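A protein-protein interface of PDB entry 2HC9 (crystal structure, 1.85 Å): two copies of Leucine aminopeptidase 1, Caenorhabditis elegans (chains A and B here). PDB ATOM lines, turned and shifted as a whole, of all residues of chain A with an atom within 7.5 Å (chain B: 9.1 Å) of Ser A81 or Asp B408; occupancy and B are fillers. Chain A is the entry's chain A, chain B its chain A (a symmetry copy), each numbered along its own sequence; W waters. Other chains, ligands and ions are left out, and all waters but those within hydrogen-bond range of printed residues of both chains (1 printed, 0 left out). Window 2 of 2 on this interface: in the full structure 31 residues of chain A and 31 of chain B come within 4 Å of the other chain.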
ATOM      1  N   LYS A  25      -7.206 -15.195  -3.818  1.00  0.00           N
ATOM      2  CA  LYS A  25      -7.803 -16.491  -4.144  1.00  0.00           C
ATOM      3  C   LYS A  25      -7.576 -16.917  -5.580  1.00  0.00           C
ATOM      4  O   LYS A  25      -7.594 -16.099  -6.505  1.00  0.00           O
ATOM      5  CB  LYS A  25      -9.286 -16.526  -3.800  1.00  0.00           C
ATOM      6  CG  LYS A  25      -9.545 -16.519  -2.283  1.00  0.00           C
ATOM      7  CD  LYS A  25     -11.016 -16.357  -1.989  1.00  0.00           C
ATOM      8  CE  LYS A  25     -11.327 -16.716  -0.539  1.00  0.00           C
ATOM      9  NZ  LYS A  25     -12.716 -16.334  -0.204  1.00  0.00           N
ATOM     10  N   PRO A  78      -6.816 -20.443  -0.847  1.00  0.00           N
ATOM     11  CA  PRO A  78      -7.833 -21.370  -1.362  1.00  0.00           C
ATOM     12  C   PRO A  78      -9.216 -20.741  -1.490  1.00  0.00           C
ATOM     13  O   PRO A  78      -9.579 -19.831  -0.725  1.00  0.00           O
ATOM     14  CB  PRO A  78      -7.833 -22.527  -0.358  1.00  0.00           C
ATOM     15  CG  PRO A  78      -7.079 -22.070   0.826  1.00  0.00           C
ATOM     16  CD  PRO A  78      -6.293 -20.831   0.478  1.00  0.00           C
ATOM     17  N   ASP A  79      -9.973 -21.224  -2.472  1.00  0.00           N
ATOM     18  CA  ASP A  79     -11.347 -20.803  -2.665  1.00  0.00           C
ATOM     19  C   ASP A  79     -12.338 -21.554  -1.770  1.00  0.00           C
ATOM     20  O   ASP A  79     -13.271 -20.957  -1.235  1.00  0.00           O
ATOM     21  CB  ASP A  79     -11.728 -20.973  -4.128  1.00  0.00           C
ATOM     22  CG  ASP A  79     -11.228 -19.824  -4.979  1.00  0.00           C
ATOM     23  OD1 ASP A  79     -11.746 -18.701  -4.835  1.00  0.00           O
ATOM     24  OD2 ASP A  79     -10.317 -20.057  -5.778  1.00  0.00           O
ATOM     25  N   ALA A  80     -12.104 -22.849  -1.600  1.00  0.00           N
ATOM     26  CA  ALA A  80     -12.996 -23.720  -0.807  1.00  0.00           C
ATOM     27  C   ALA A  80     -12.811 -23.508   0.691  1.00  0.00           C
ATOM     28  O   ALA A  80     -11.714 -23.213   1.141  1.00  0.00           O
ATOM     29  CB  ALA A  80     -12.733 -25.173  -1.141  1.00  0.00           C
ATOM     30  N   SER A  81     -13.877 -23.684   1.468  1.00  0.00           N
ATOM     31  CA  SER A  81     -13.745 -23.672   2.924  1.00  0.00           C
ATOM     32  C   SER A  81     -14.829 -24.524   3.563  1.00  0.00           C
ATOM     33  O   SER A  81     -15.934 -24.654   3.023  1.00  0.00           O
ATOM     34  CB  SER A  81     -13.802 -22.238   3.501  1.00  0.00           C
ATOM     35  OG  SER A  81     -15.034 -21.648   3.160  1.00  0.00           O
ATOM     36  N   SER A  82     -14.511 -25.077   4.726  1.00  0.00           N
ATOM     37  CA  SER A  82     -15.489 -25.846   5.498  1.00  0.00           C
ATOM     38  C   SER A  82     -16.407 -24.912   6.269  1.00  0.00           C
ATOM     39  O   SER A  82     -16.101 -23.722   6.522  1.00  0.00           O
ATOM     40  CB  SER A  82     -14.764 -26.736   6.521  1.00  0.00           C
ATOM     41  OG  SER A  82     -14.153 -25.903   7.511  1.00  0.00           O
ATOM     42  N   ARG A  83     -17.521 -25.473   6.726  1.00  0.00           N
ATOM     43  CA  ARG A  83     -18.480 -24.645   7.430  1.00  0.00           C
ATOM     44  C   ARG A  83     -17.961 -24.095   8.759  1.00  0.00           C
ATOM     45  O   ARG A  83     -18.368 -23.012   9.150  1.00  0.00           O
ATOM     46  CB  ARG A  83     -19.838 -25.341   7.577  1.00  0.00           C
ATOM     47  CG  ARG A  83     -19.810 -26.601   8.421  1.00  0.00           C
ATOM     48  CD  ARG A  83     -21.170 -27.313   8.365  1.00  0.00           C
ATOM     49  NE  ARG A  83     -21.351 -28.185   9.525  1.00  0.00           N
ATOM     50  CZ  ARG A  83     -21.814 -27.786  10.708  1.00  0.00           C
ATOM     51  NH1 ARG A  83     -21.932 -28.658  11.700  1.00  0.00           N
ATOM     52  NH2 ARG A  83     -22.153 -26.522  10.911  1.00  0.00           N
ATOM     53  N   GLY A  84     -17.029 -24.794   9.414  1.00  0.00           N
ATOM     54  CA  GLY A  84     -16.432 -24.307  10.683  1.00  0.00           C
ATOM     55  C   GLY A  84     -15.340 -23.249  10.494  1.00  0.00           C
ATOM     56  O   GLY A  84     -14.958 -22.552  11.454  1.00  0.00           O
ATOM     57  N   ASN A  85     -14.880 -23.096   9.251  1.00  0.00           N
ATOM     58  CA  ASN A  85     -13.826 -22.143   8.899  1.00  0.00           C
ATOM     59  C   ASN A  85     -14.464 -20.789   8.560  1.00  0.00           C
ATOM     60  O   ASN A  85     -15.679 -20.657   8.569  1.00  0.00           O
ATOM     61  CB  ASN A  85     -13.063 -22.699   7.695  1.00  0.00           C
ATOM     62  CG  ASN A  85     -11.701 -22.019   7.463  1.00  0.00           C
ATOM     63  OD1 ASN A  85     -11.334 -21.032   8.129  1.00  0.00           O
ATOM     64  ND2 ASN A  85     -10.960 -22.547   6.492  1.00  0.00           N
ATOM     65  N   THR A  86     -13.648 -19.782   8.280  1.00  0.00           N
ATOM     66  CA  THR A  86     -14.138 -18.577   7.602  1.00  0.00           C
ATOM     67  C   THR A  86     -14.040 -18.782   6.084  1.00  0.00           C
ATOM     68  O   THR A  86     -13.017 -19.284   5.578  1.00  0.00           O
ATOM     69  CB  THR A  86     -13.326 -17.314   8.048  1.00  0.00           C
ATOM     70  OG1 THR A  86     -13.630 -16.209   7.177  1.00  0.00           O
ATOM     71  CG2 THR A  86     -11.802 -17.603   8.023  1.00  0.00           C
ATOM     72  N   PRO A  87     -15.080 -18.365   5.340  1.00  0.00           N
ATOM     73  CA  PRO A  87     -14.976 -18.479   3.879  1.00  0.00           C
ATOM     74  C   PRO A  87     -13.934 -17.531   3.271  1.00  0.00           C
ATOM     75  O   PRO A  87     -13.550 -17.691   2.112  1.00  0.00           O
ATOM     76  CB  PRO A  87     -16.375 -18.110   3.385  1.00  0.00           C
ATOM     77  CG  PRO A  87     -16.956 -17.250   4.462  1.00  0.00           C
ATOM     78  CD  PRO A  87     -16.350 -17.748   5.772  1.00  0.00           C
ATOM     79  N   THR A  88     -13.452 -16.582   4.069  1.00  0.00           N
ATOM     80  CA  THR A  88     -12.330 -15.717   3.638  1.00  0.00           C
ATOM     81  C   THR A  88     -11.021 -16.481   3.528  1.00  0.00           C
ATOM     82  O   THR A  88     -10.107 -16.043   2.822  1.00  0.00           O
ATOM     83  CB  THR A  88     -12.100 -14.548   4.615  1.00  0.00           C
ATOM     84  OG1 THR A  88     -11.513 -15.056   5.820  1.00  0.00           O
ATOM     85  CG2 THR A  88     -13.396 -13.812   4.959  1.00  0.00           C
ATOM     86  N   ASN A  89     -10.902 -17.593   4.270  1.00  0.00           N
ATOM     87  CA  ASN A  89      -9.620 -18.350   4.360  1.00  0.00           C
ATOM     88  C   ASN A  89      -8.434 -17.448   4.762  1.00  0.00           C
ATOM     89  O   ASN A  89      -7.295 -17.660   4.344  1.00  0.00           O
ATOM     90  CB  ASN A  89      -9.305 -19.072   3.042  1.00  0.00           C
ATOM     91  CG  ASN A  89     -10.146 -20.316   2.839  1.00  0.00           C
ATOM     92  OD1 ASN A  89     -10.683 -20.545   1.754  1.00  0.00           O
ATOM     93  ND2 ASN A  89     -10.286 -21.108   3.887  1.00  0.00           N
ATOM     94  N   SER A  92      -4.951 -18.655   5.872  1.00  0.00           N
ATOM     95  CA  SER A  92      -4.026 -19.138   4.846  1.00  0.00           C
ATOM     96  C   SER A  92      -3.022 -18.067   4.437  1.00  0.00           C
ATOM     97  O   SER A  92      -1.868 -18.372   4.131  1.00  0.00           O
ATOM     98  CB  SER A  92      -4.780 -19.614   3.594  1.00  0.00           C
ATOM     99  OG  SER A  92      -5.600 -20.734   3.871  1.00  0.00           O
ATOM    100  N   LYS A  95      -0.487 -17.951   7.254  1.00  0.00           N
ATOM    101  CA  LYS A  95       0.381 -19.138   7.189  1.00  0.00           C
ATOM    102  C   LYS A  95       1.511 -19.012   6.155  1.00  0.00           C
ATOM    103  O   LYS A  95       2.654 -19.418   6.400  1.00  0.00           O
ATOM    104  CB  LYS A  95      -0.471 -20.380   6.871  1.00  0.00           C
ATOM    105  CG  LYS A  95       0.336 -21.671   6.806  1.00  0.00           C
ATOM    106  CD  LYS A  95      -0.504 -22.878   6.497  1.00  0.00           C
ATOM    107  CE  LYS A  95      -1.014 -22.845   5.063  1.00  0.00           C
ATOM    108  NZ  LYS A  95      -2.486 -22.604   5.057  1.00  0.00           N
ATOM    109  N   LEU B 404     -16.985 -28.293  16.384  1.00  0.00           N
ATOM    110  CA  LEU B 404     -16.606 -27.661  15.110  1.00  0.00           C
ATOM    111  C   LEU B 404     -16.330 -28.691  14.039  1.00  0.00           C
ATOM    112  O   LEU B 404     -15.645 -29.709  14.288  1.00  0.00           O
ATOM    113  CB  LEU B 404     -15.330 -26.815  15.264  1.00  0.00           C
ATOM    114  CG  LEU B 404     -15.430 -25.461  15.963  1.00  0.00           C
ATOM    115  CD1 LEU B 404     -14.002 -24.927  16.252  1.00  0.00           C
ATOM    116  CD2 LEU B 404     -16.238 -24.491  15.097  1.00  0.00           C
ATOM    117  N   PHE B 405     -16.847 -28.404  12.847  1.00  0.00           N
ATOM    118  CA  PHE B 405     -16.566 -29.218  11.676  1.00  0.00           C
ATOM    119  C   PHE B 405     -15.655 -28.426  10.737  1.00  0.00           C
ATOM    120  O   PHE B 405     -16.114 -27.529  10.011  1.00  0.00           O
ATOM    121  CB  PHE B 405     -17.864 -29.591  10.942  1.00  0.00           C
ATOM    122  CG  PHE B 405     -17.632 -30.478   9.731  1.00  0.00           C
ATOM    123  CD1 PHE B 405     -17.443 -31.848   9.885  1.00  0.00           C
ATOM    124  CD2 PHE B 405     -17.570 -29.940   8.448  1.00  0.00           C
ATOM    125  CE1 PHE B 405     -17.205 -32.676   8.757  1.00  0.00           C
ATOM    126  CE2 PHE B 405     -17.342 -30.752   7.319  1.00  0.00           C
ATOM    127  CZ  PHE B 405     -17.155 -32.125   7.488  1.00  0.00           C
ATOM    128  N   ALA B 406     -14.377 -28.774  10.719  1.00  0.00           N
ATOM    129  CA  ALA B 406     -13.424 -28.027   9.865  1.00  0.00           C
ATOM    130  C   ALA B 406     -12.252 -28.909   9.396  1.00  0.00           C
ATOM    131  O   ALA B 406     -11.136 -28.746   9.868  1.00  0.00           O
ATOM    132  CB  ALA B 406     -12.923 -26.769  10.610  1.00  0.00           C
ATOM    133  N   PRO B 407     -12.513 -29.849   8.458  1.00  0.00           N
ATOM    134  CA  PRO B 407     -11.425 -30.712   8.017  1.00  0.00           C
ATOM    135  C   PRO B 407     -10.294 -29.882   7.391  1.00  0.00           C
ATOM    136  O   PRO B 407      -9.128 -30.197   7.596  1.00  0.00           O
ATOM    137  CB  PRO B 407     -12.080 -31.621   6.973  1.00  0.00           C
ATOM    138  CG  PRO B 407     -13.578 -31.587   7.295  1.00  0.00           C
ATOM    139  CD  PRO B 407     -13.797 -30.167   7.781  1.00  0.00           C
ATOM    140  N   ASP B 408     -10.633 -28.812   6.674  1.00  0.00           N
ATOM    141  CA  ASP B 408      -9.573 -27.946   6.110  1.00  0.00           C
ATOM    142  C   ASP B 408      -8.626 -27.363   7.159  1.00  0.00           C
ATOM    143  O   ASP B 408      -7.407 -27.300   6.943  1.00  0.00           O
ATOM    144  CB  ASP B 408     -10.147 -26.847   5.199  1.00  0.00           C
ATOM    145  CG  ASP B 408     -11.241 -26.000   5.874  1.00  0.00           C
ATOM    146  OD1 ASP B 408     -11.621 -26.248   7.047  1.00  0.00           O
ATOM    147  OD2 ASP B 408     -11.739 -25.066   5.203  1.00  0.00           O
ATOM    148  N   LEU B 409      -9.162 -26.956   8.299  1.00  0.00           N
ATOM    149  CA  LEU B 409      -8.321 -26.352   9.349  1.00  0.00           C
ATOM    150  C   LEU B 409      -7.598 -27.394  10.200  1.00  0.00           C
ATOM    151  O   LEU B 409      -6.492 -27.137  10.659  1.00  0.00           O
ATOM    152  CB  LEU B 409      -9.151 -25.460  10.273  1.00  0.00           C
ATOM    153  CG  LEU B 409      -9.740 -24.186   9.647  1.00  0.00           C
ATOM    154  CD1 LEU B 409     -10.515 -23.442  10.766  1.00  0.00           C
ATOM    155  CD2 LEU B 409      -8.617 -23.300   9.053  1.00  0.00           C
ATOM    156  N   PHE B 410      -8.230 -28.547  10.426  1.00  0.00           N
ATOM    157  CA  PHE B 410      -7.778 -29.452  11.490  1.00  0.00           C
ATOM    158  C   PHE B 410      -7.191 -30.782  11.019  1.00  0.00           C
ATOM    159  O   PHE B 410      -6.470 -31.429  11.762  1.00  0.00           O
ATOM    160  CB  PHE B 410      -8.912 -29.737  12.491  1.00  0.00           C
ATOM    161  CG  PHE B 410      -9.530 -28.504  13.119  1.00  0.00           C
ATOM    162  CD1 PHE B 410      -8.765 -27.359  13.389  1.00  0.00           C
ATOM    163  CD2 PHE B 410     -10.872 -28.532  13.510  1.00  0.00           C
ATOM    164  CE1 PHE B 410      -9.334 -26.232  13.995  1.00  0.00           C
ATOM    165  CE2 PHE B 410     -11.476 -27.410  14.140  1.00  0.00           C
ATOM    166  CZ  PHE B 410     -10.699 -26.252  14.389  1.00  0.00           C
ATOM    167  N   PHE B 411      -7.497 -31.213   9.799  1.00  0.00           N
ATOM    168  CA  PHE B 411      -7.047 -32.552   9.364  1.00  0.00           C
ATOM    169  C   PHE B 411      -5.522 -32.633   9.239  1.00  0.00           C
ATOM    170  O   PHE B 411      -4.904 -33.713   9.389  1.00  0.00           O
ATOM    171  CB  PHE B 411      -7.780 -33.004   8.087  1.00  0.00           C
ATOM    172  CG  PHE B 411      -7.364 -34.380   7.597  1.00  0.00           C
ATOM    173  CD1 PHE B 411      -7.620 -35.512   8.369  1.00  0.00           C
ATOM    174  CD2 PHE B 411      -6.695 -34.529   6.391  1.00  0.00           C
ATOM    175  CE1 PHE B 411      -7.218 -36.778   7.935  1.00  0.00           C
ATOM    176  CE2 PHE B 411      -6.304 -35.795   5.937  1.00  0.00           C
ATOM    177  CZ  PHE B 411      -6.567 -36.915   6.711  1.00  0.00           C
ATOM    178  N   GLY B 412      -4.903 -31.479   9.021  1.00  0.00           N
ATOM    179  CA  GLY B 412      -3.445 -31.389   9.030  1.00  0.00           C
ATOM    180  C   GLY B 412      -2.805 -31.813  10.352  1.00  0.00           C
ATOM    181  O   GLY B 412      -1.623 -32.176  10.382  1.00  0.00           O
ATOM    182  N   ASP B 413      -3.570 -31.786  11.443  1.00  0.00           N
ATOM    183  CA  ASP B 413      -3.112 -32.385  12.712  1.00  0.00           C
ATOM    184  C   ASP B 413      -2.718 -33.879  12.560  1.00  0.00           C
ATOM    185  O   ASP B 413      -1.919 -34.395  13.355  1.00  0.00           O
ATOM    186  CB  ASP B 413      -4.186 -32.240  13.797  1.00  0.00           C
ATOM    187  CG  ASP B 413      -4.406 -30.789  14.228  1.00  0.00           C
ATOM    188  OD1 ASP B 413      -3.531 -29.909  13.958  1.00  0.00           O
ATOM    189  OD2 ASP B 413      -5.457 -30.539  14.865  1.00  0.00           O
ATOM    190  N   ASP B 430      -4.014 -28.070  16.218  1.00  0.00           N
ATOM    191  CA  ASP B 430      -4.879 -26.905  16.014  1.00  0.00           C
ATOM    192  C   ASP B 430      -6.338 -27.190  16.349  1.00  0.00           C
ATOM    193  O   ASP B 430      -7.039 -26.296  16.754  1.00  0.00           O
ATOM    194  CB  ASP B 430      -4.792 -26.420  14.581  1.00  0.00           C
ATOM    195  CG  ASP B 430      -3.524 -25.614  14.311  1.00  0.00           C
ATOM    196  OD1 ASP B 430      -2.880 -25.149  15.270  1.00  0.00           O
ATOM    197  OD2 ASP B 430      -3.192 -25.449  13.126  1.00  0.00           O
ATOM    198  N   LEU B 439     -12.339 -36.665  12.813  1.00  0.00           N
ATOM    199  CA  LEU B 439     -11.867 -36.436  11.436  1.00  0.00           C
ATOM    200  C   LEU B 439     -11.058 -37.607  10.912  1.00  0.00           C
ATOM    201  O   LEU B 439     -11.042 -37.845   9.708  1.00  0.00           O
ATOM    202  CB  LEU B 439     -11.022 -35.148  11.355  1.00  0.00           C
ATOM    203  CG  LEU B 439     -11.819 -33.843  11.523  1.00  0.00           C
ATOM    204  CD1 LEU B 439     -10.813 -32.658  11.575  1.00  0.00           C
ATOM    205  CD2 LEU B 439     -12.823 -33.683  10.385  1.00  0.00           C
ATOM    206  N   PHE B 447     -14.982 -37.044   4.401  1.00  0.00           N
ATOM    207  CA  PHE B 447     -15.603 -36.199   5.426  1.00  0.00           C
ATOM    208  C   PHE B 447     -17.119 -36.054   5.241  1.00  0.00           C
ATOM    209  O   PHE B 447     -17.703 -35.053   5.649  1.00  0.00           O
ATOM    210  CB  PHE B 447     -14.891 -34.843   5.549  1.00  0.00           C
ATOM    211  CG  PHE B 447     -13.415 -34.978   5.780  1.00  0.00           C
ATOM    212  CD1 PHE B 447     -12.932 -35.414   7.020  1.00  0.00           C
ATOM    213  CD2 PHE B 447     -12.507 -34.691   4.757  1.00  0.00           C
ATOM    214  CE1 PHE B 447     -11.522 -35.584   7.225  1.00  0.00           C
ATOM    215  CE2 PHE B 447     -11.108 -34.856   4.960  1.00  0.00           C
ATOM    216  CZ  PHE B 447     -10.635 -35.296   6.193  1.00  0.00           C
HETATM  217  O   HOH W   1      -9.973 -24.182   3.257  1.00  0.00           O
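Of the printed residues of chain B, Ser A81 touches Asp B408 (3.3 Å). Of the printed residues of chain A, Asp B408 touches Ser A81, Ser A82 and Asn A85. Ser A82 touches just these residues of chain B: Phe B405 (3.6 Å), Ala B406 (3.3 Å), Pro B407 (3.8 Å) and Asp B408 (2.6 Å). No residue of chain B comes within 4 Å of Pro A87. Printed residues of chain A within 4 Å of Leu B409: Asn A85 (3.6 Å). Printed residues of chain B within 4 Å of Gly A84: Phe B405 (2.9 Å). The nearest printed residue of chain B that does not touch Asn A85 is Ala B406 (4.4 Å).
The side-chain carboxylate (OD1) of Asp B408 lies within hydrogen-bond range of the side-chain hydroxyl (OG) of Ser A82 (2.6 Å). The backbone carbonyl oxygen (O) of Phe B405 lies within hydrogen-bond range of the backbone NH (N) of Gly A84, 2.9 Å away. The side-chain carboxylate (OD2) of Asp B408 sits at hydrogen-bond distance from the side-chain amide nitrogen (ND2) of Asn A85 (2.9 Å).
Of the 15 printed residues of chain A, 4 touch a printed residue of chain B. Printed residues of chain B that touch a printed residue of chain A: Phe B405, Ala B406, Pro B407, Asp B408 and Leu B409. Along chain B the printed residues that touch a printed residue of chain A span positions 405 to 409. Among the printed residues, no Asp or Glu carboxylate lies within 4 Å of a Lys or Arg side-chain nitrogen of the other chain.
The backbone NH (N) of Asn A85 sits at hydrogen-bond distance from the side-chain hydroxyl (OG) of Ser A82 (3.4 Å). The side-chain amide nitrogen (ND2) of Asn A85 lies close to the side-chain amide nitrogen (ND2) of Asn A89 (3.1 Å).
No position is printed for both chains.
Water W1 lies within hydrogen-bond range of the side-chain carboxylate (OD2) of Asp B408 (2.8 Å), the backbone carbonyl oxygen (O) of Ala A80 (2.9 Å) and the side-chain amide nitrogen (ND2) of Asn A89 (3.2 Å).
Ser A81 touches Asp B408. Ser A82 touches Phe B405 (OG to O, 3.6 Å). Ala B406 touches Ser A82. Ser A82 touches Pro B407 (CB to CD, 3.8 Å). ND2 of Asn A85 touches CD2 of Leu B409 (3.6 Å).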
